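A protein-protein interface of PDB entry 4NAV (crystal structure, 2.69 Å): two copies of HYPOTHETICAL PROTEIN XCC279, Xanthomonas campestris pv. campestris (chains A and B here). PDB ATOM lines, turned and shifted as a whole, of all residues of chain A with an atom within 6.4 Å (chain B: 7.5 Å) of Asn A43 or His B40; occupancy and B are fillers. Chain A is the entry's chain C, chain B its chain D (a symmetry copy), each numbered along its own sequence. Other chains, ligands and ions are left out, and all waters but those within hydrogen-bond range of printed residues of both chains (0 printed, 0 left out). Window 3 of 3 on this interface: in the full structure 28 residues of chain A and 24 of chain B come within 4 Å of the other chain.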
ATOM      1  N   TYR A  37      20.455 -28.453   2.016  1.00  0.00           N
ATOM      2  CA  TYR A  37      21.251 -27.729   2.978  1.00  0.00           C
ATOM      3  C   TYR A  37      21.426 -28.605   4.226  1.00  0.00           C
ATOM      4  O   TYR A  37      20.448 -28.947   4.894  1.00  0.00           O
ATOM      5  CB  TYR A  37      20.580 -26.388   3.296  1.00  0.00           C
ATOM      6  CG  TYR A  37      20.393 -25.534   2.048  1.00  0.00           C
ATOM      7  CD1 TYR A  37      21.285 -24.527   1.740  1.00  0.00           C
ATOM      8  CD2 TYR A  37      19.319 -25.742   1.177  1.00  0.00           C
ATOM      9  CE1 TYR A  37      21.127 -23.756   0.600  1.00  0.00           C
ATOM     10  CE2 TYR A  37      19.161 -24.981   0.025  1.00  0.00           C
ATOM     11  CZ  TYR A  37      20.082 -23.993  -0.263  1.00  0.00           C
ATOM     12  OH  TYR A  37      19.946 -23.231  -1.412  1.00  0.00           O
ATOM     13  N   TYR A  38      22.670 -28.993   4.489  1.00  0.00           N
ATOM     14  CA  TYR A  38      23.018 -29.795   5.648  1.00  0.00           C
ATOM     15  C   TYR A  38      23.621 -28.914   6.716  1.00  0.00           C
ATOM     16  O   TYR A  38      24.545 -28.139   6.457  1.00  0.00           O
ATOM     17  CB  TYR A  38      24.061 -30.849   5.305  1.00  0.00           C
ATOM     18  CG  TYR A  38      23.547 -32.137   4.713  1.00  0.00           C
ATOM     19  CD1 TYR A  38      23.824 -33.354   5.326  1.00  0.00           C
ATOM     20  CD2 TYR A  38      22.830 -32.142   3.535  1.00  0.00           C
ATOM     21  CE1 TYR A  38      23.393 -34.549   4.792  1.00  0.00           C
ATOM     22  CE2 TYR A  38      22.403 -33.326   2.981  1.00  0.00           C
ATOM     23  CZ  TYR A  38      22.688 -34.531   3.622  1.00  0.00           C
ATOM     24  OH  TYR A  38      22.260 -35.724   3.107  1.00  0.00           O
ATOM     25  N   ASP A  39      23.102 -29.059   7.923  1.00  0.00           N
ATOM     26  CA  ASP A  39      23.538 -28.283   9.075  1.00  0.00           C
ATOM     27  C   ASP A  39      24.541 -29.128   9.896  1.00  0.00           C
ATOM     28  O   ASP A  39      24.842 -30.244   9.506  1.00  0.00           O
ATOM     29  CB  ASP A  39      22.232 -27.821   9.735  1.00  0.00           C
ATOM     30  CG  ASP A  39      22.083 -28.193  11.167  1.00  0.00           C
ATOM     31  OD1 ASP A  39      23.072 -28.547  11.820  1.00  0.00           O
ATOM     32  OD2 ASP A  39      20.923 -28.101  11.627  1.00  0.00           O
ATOM     33  N   HIS A  40      25.128 -28.576  10.953  1.00  0.00           N
ATOM     34  CA  HIS A  40      26.258 -29.250  11.634  1.00  0.00           C
ATOM     35  C   HIS A  40      25.890 -30.608  12.284  1.00  0.00           C
ATOM     36  O   HIS A  40      26.768 -31.406  12.626  1.00  0.00           O
ATOM     37  CB  HIS A  40      26.931 -28.324  12.657  1.00  0.00           C
ATOM     38  CG  HIS A  40      26.125 -28.102  13.891  1.00  0.00           C
ATOM     39  ND1 HIS A  40      26.185 -28.936  14.989  1.00  0.00           N
ATOM     40  CD2 HIS A  40      25.227 -27.140  14.200  1.00  0.00           C
ATOM     41  CE1 HIS A  40      25.368 -28.492  15.926  1.00  0.00           C
ATOM     42  NE2 HIS A  40      24.778 -27.402  15.472  1.00  0.00           N
ATOM     43  N   ALA A  41      24.589 -30.860  12.421  1.00  0.00           N
ATOM     44  CA  ALA A  41      24.071 -32.092  13.000  1.00  0.00           C
ATOM     45  C   ALA A  41      23.402 -32.958  11.940  1.00  0.00           C
ATOM     46  O   ALA A  41      22.628 -33.850  12.271  1.00  0.00           O
ATOM     47  CB  ALA A  41      23.074 -31.751  14.098  1.00  0.00           C
ATOM     48  N   GLY A  42      23.687 -32.698  10.665  1.00  0.00           N
ATOM     49  CA  GLY A  42      23.121 -33.497   9.581  1.00  0.00           C
ATOM     50  C   GLY A  42      21.652 -33.232   9.262  1.00  0.00           C
ATOM     51  O   GLY A  42      21.124 -33.822   8.315  1.00  0.00           O
ATOM     52  N   ASN A  43      20.992 -32.358  10.033  1.00  0.00           N
ATOM     53  CA  ASN A  43      19.635 -31.909   9.704  1.00  0.00           C
ATOM     54  C   ASN A  43      19.543 -31.196   8.341  1.00  0.00           C
ATOM     55  O   ASN A  43      20.376 -30.347   8.011  1.00  0.00           O
ATOM     56  CB  ASN A  43      19.105 -30.958  10.786  1.00  0.00           C
ATOM     57  CG  ASN A  43      18.828 -31.654  12.093  1.00  0.00           C
ATOM     58  OD1 ASN A  43      18.864 -31.009  13.127  1.00  0.00           O
ATOM     59  ND2 ASN A  43      18.572 -32.973  12.067  1.00  0.00           N
ATOM     60  N   GLU A  44      18.494 -31.507   7.585  1.00  0.00           N
ATOM     61  CA  GLU A  44      18.374 -31.050   6.215  1.00  0.00           C
ATOM     62  C   GLU A  44      17.295 -29.968   5.994  1.00  0.00           C
ATOM     63  O   GLU A  44      16.270 -29.974   6.661  1.00  0.00           O
ATOM     64  CB  GLU A  44      18.104 -32.252   5.315  1.00  0.00           C
ATOM     65  CG  GLU A  44      19.235 -33.284   5.317  1.00  0.00           C
ATOM     66  CD  GLU A  44      18.923 -34.480   4.439  1.00  0.00           C
ATOM     67  OE1 GLU A  44      19.454 -35.591   4.657  1.00  0.00           O
ATOM     68  OE2 GLU A  44      18.127 -34.305   3.509  1.00  0.00           O
ATOM     69  N   SER A  45      17.552 -29.035   5.069  1.00  0.00           N
ATOM     70  CA  SER A  45      16.547 -28.093   4.601  1.00  0.00           C
ATOM     71  C   SER A  45      16.523 -28.073   3.080  1.00  0.00           C
ATOM     72  O   SER A  45      17.512 -28.416   2.439  1.00  0.00           O
ATOM     73  CB  SER A  45      16.854 -26.679   5.071  1.00  0.00           C
ATOM     74  OG  SER A  45      16.826 -26.569   6.465  1.00  0.00           O
ATOM     75  N   SER A  74      11.243 -37.249   4.679  1.00  0.00           N
ATOM     76  CA  SER A  74      11.424 -35.898   5.234  1.00  0.00           C
ATOM     77  C   SER A  74      10.135 -35.233   5.766  1.00  0.00           C
ATOM     78  O   SER A  74       9.125 -35.166   5.062  1.00  0.00           O
ATOM     79  CB  SER A  74      12.105 -34.977   4.192  1.00  0.00           C
ATOM     80  OG  SER A  74      11.185 -34.486   3.236  1.00  0.00           O
ATOM     81  N   LEU A  75      10.184 -34.703   6.992  1.00  0.00           N
ATOM     82  CA  LEU A  75       9.062 -33.909   7.524  1.00  0.00           C
ATOM     83  C   LEU A  75       8.875 -32.598   6.725  1.00  0.00           C
ATOM     84  O   LEU A  75       7.762 -32.055   6.701  1.00  0.00           O
ATOM     85  CB  LEU A  75       9.225 -33.619   9.023  1.00  0.00           C
ATOM     86  N   SER A  76       9.947 -32.115   6.062  1.00  0.00           N
ATOM     87  CA  SER A  76       9.906 -30.907   5.210  1.00  0.00           C
ATOM     88  C   SER A  76       8.778 -30.982   4.218  1.00  0.00           C
ATOM     89  O   SER A  76       7.941 -30.082   4.114  1.00  0.00           O
ATOM     90  CB  SER A  76      11.191 -30.745   4.376  1.00  0.00           C
ATOM     91  OG  SER A  76      12.335 -30.468   5.154  1.00  0.00           O
ATOM     92  N   TYR B  38      12.523 -24.703   3.875  1.00  0.00           N
ATOM     93  CA  TYR B  38      11.843 -25.491   4.877  1.00  0.00           C
ATOM     94  C   TYR B  38      12.870 -26.333   5.566  1.00  0.00           C
ATOM     95  O   TYR B  38      13.647 -27.038   4.916  1.00  0.00           O
ATOM     96  CB  TYR B  38      10.824 -26.407   4.231  1.00  0.00           C
ATOM     97  CG  TYR B  38       9.484 -25.774   3.935  1.00  0.00           C
ATOM     98  CD1 TYR B  38       8.329 -26.331   4.440  1.00  0.00           C
ATOM     99  CD2 TYR B  38       9.367 -24.675   3.104  1.00  0.00           C
ATOM    100  CE1 TYR B  38       7.090 -25.799   4.153  1.00  0.00           C
ATOM    101  CE2 TYR B  38       8.131 -24.121   2.816  1.00  0.00           C
ATOM    102  CZ  TYR B  38       6.998 -24.694   3.343  1.00  0.00           C
ATOM    103  OH  TYR B  38       5.756 -24.170   3.067  1.00  0.00           O
ATOM    104  N   ASP B  39      12.853 -26.302   6.891  1.00  0.00           N
ATOM    105  CA  ASP B  39      13.762 -27.147   7.694  1.00  0.00           C
ATOM    106  C   ASP B  39      13.032 -28.426   8.100  1.00  0.00           C
ATOM    107  O   ASP B  39      11.872 -28.618   7.740  1.00  0.00           O
ATOM    108  CB  ASP B  39      14.352 -26.358   8.884  1.00  0.00           C
ATOM    109  CG  ASP B  39      13.473 -26.374  10.115  1.00  0.00           C
ATOM    110  OD1 ASP B  39      13.930 -26.833  11.155  1.00  0.00           O
ATOM    111  OD2 ASP B  39      12.339 -25.884  10.061  1.00  0.00           O
ATOM    112  N   HIS B  40      13.697 -29.312   8.821  1.00  0.00           N
ATOM    113  CA  HIS B  40      13.118 -30.643   9.083  1.00  0.00           C
ATOM    114  C   HIS B  40      11.806 -30.631   9.923  1.00  0.00           C
ATOM    115  O   HIS B  40      11.093 -31.633   9.983  1.00  0.00           O
ATOM    116  CB  HIS B  40      14.166 -31.560   9.716  1.00  0.00           C
ATOM    117  CG  HIS B  40      14.511 -31.192  11.125  1.00  0.00           C
ATOM    118  ND1 HIS B  40      13.807 -31.667  12.211  1.00  0.00           N
ATOM    119  CD2 HIS B  40      15.477 -30.386  11.625  1.00  0.00           C
ATOM    120  CE1 HIS B  40      14.332 -31.180  13.321  1.00  0.00           C
ATOM    121  NE2 HIS B  40      15.351 -30.404  12.993  1.00  0.00           N
ATOM    122  N   ALA B  41      11.502 -29.500  10.554  1.00  0.00           N
ATOM    123  CA  ALA B  41      10.304 -29.350  11.367  1.00  0.00           C
ATOM    124  C   ALA B  41       9.298 -28.432  10.695  1.00  0.00           C
ATOM    125  O   ALA B  41       8.399 -27.905  11.350  1.00  0.00           O
ATOM    126  CB  ALA B  41      10.680 -28.794  12.739  1.00  0.00           C
ATOM    127  N   GLY B  42       9.464 -28.191   9.396  1.00  0.00           N
ATOM    128  CA  GLY B  42       8.544 -27.314   8.654  1.00  0.00           C
ATOM    129  C   GLY B  42       8.708 -25.824   8.882  1.00  0.00           C
ATOM    130  O   GLY B  42       7.998 -25.029   8.242  1.00  0.00           O
ATOM    131  N   ASN B  43       9.613 -25.430   9.785  1.00  0.00           N
ATOM    132  CA  ASN B  43       9.923 -24.006   9.984  1.00  0.00           C
ATOM    133  C   ASN B  43      10.528 -23.349   8.733  1.00  0.00           C
ATOM    134  O   ASN B  43      11.380 -23.933   8.064  1.00  0.00           O
ATOM    135  CB  ASN B  43      10.836 -23.820  11.196  1.00  0.00           C
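The backbone carbonyl oxygen of Glu A44 sits at hydrogen-bond distance from the backbone NH of His B40 (3.4 Å). The side-chain hydroxyl (OG) of Ser A76 lies within hydrogen-bond range of the backbone carbonyl oxygen (O) of Asp B39.
The backbone carbonyl oxygen of Tyr A37 lies within hydrogen-bond range of the backbone NH of Ser A45 (2.9 Å). The side-chain carboxylate of Glu A44 lies within hydrogen-bond range of the side-chain hydroxyl of Tyr A38. N of Asn B43 sits at hydrogen-bond distance from OD2 of Asp B39 (2.8 Å).
His B40 touches Asn A43 (NE2 to OD1, 3.6 Å). Asp B39 touches Glu A44. Tyr B38 touches Ser A45 (O to CA, 3.1 Å). Asp B39 touches Ser A45. His B40 touches Leu A75. Ser A76 touches Tyr B38.
Tyr A38 touches none of the printed residues of chain B. No residue of chain B comes within 4 Å of Gly A42. Asn A43 touches one residue of chain B. Of the printed residues of chain B, Leu A75 touches His B40 (2.9 Å). Printed residues of chain B within 4 Å of Ser A76: Tyr B38 and Asp B39. Of the printed residues of chain A, Tyr B38 touches Ser A45 (3.1 Å) and Ser A76 (3.7 Å). Of the printed residues of chain A, Asp B39 touches Glu A44 (3.9 Å), Ser A45 (3.4 Å) and Ser A76 (3.2 Å). Of the printed residues of chain A, His B40 touches Asn A43, Glu A44 and Leu A75. Ala B41 touches none of the printed residues of chain A. The nearest residue of chain B that does not touch Asn A43 is Asp B39 (6.6 Å). The nearest printed residue of chain A that does not touch His B40 is Ser A76 (4.01 Å).
Of the 12 printed residues of chain A, 5 touch a printed residue of chain B. Printed residues of chain A that touch a printed residue of chain B: Asn A43, Glu A44, Ser A45, Leu A75 and Ser A76. Hydrophobic or aromatic side chains of chain A within 4 Å of the printed part of chain B: Leu A75. Of the 6 printed residues of chain B, 3 touch a printed residue of chain A. Printed residues of chain B that touch a printed residue of chain A: Tyr B38, Asp B39 and His B40. Hydrophobic or aromatic side chains of chain B that line the printed part of chain A: Tyr B38 and His B40. Among the printed residues, 8 pairs touch across the chains. Among the printed residues, no Asp or Glu carboxylate lies within 4 Å of a Lys or Arg side-chain nitrogen of the other chain.
Asn A43 touches His B40, but with the chains exchanged His A40 does not touch Asn B43 (14.8 Å). Positions printed for both chains: 38, 39, 40, 41, 42 and 43.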
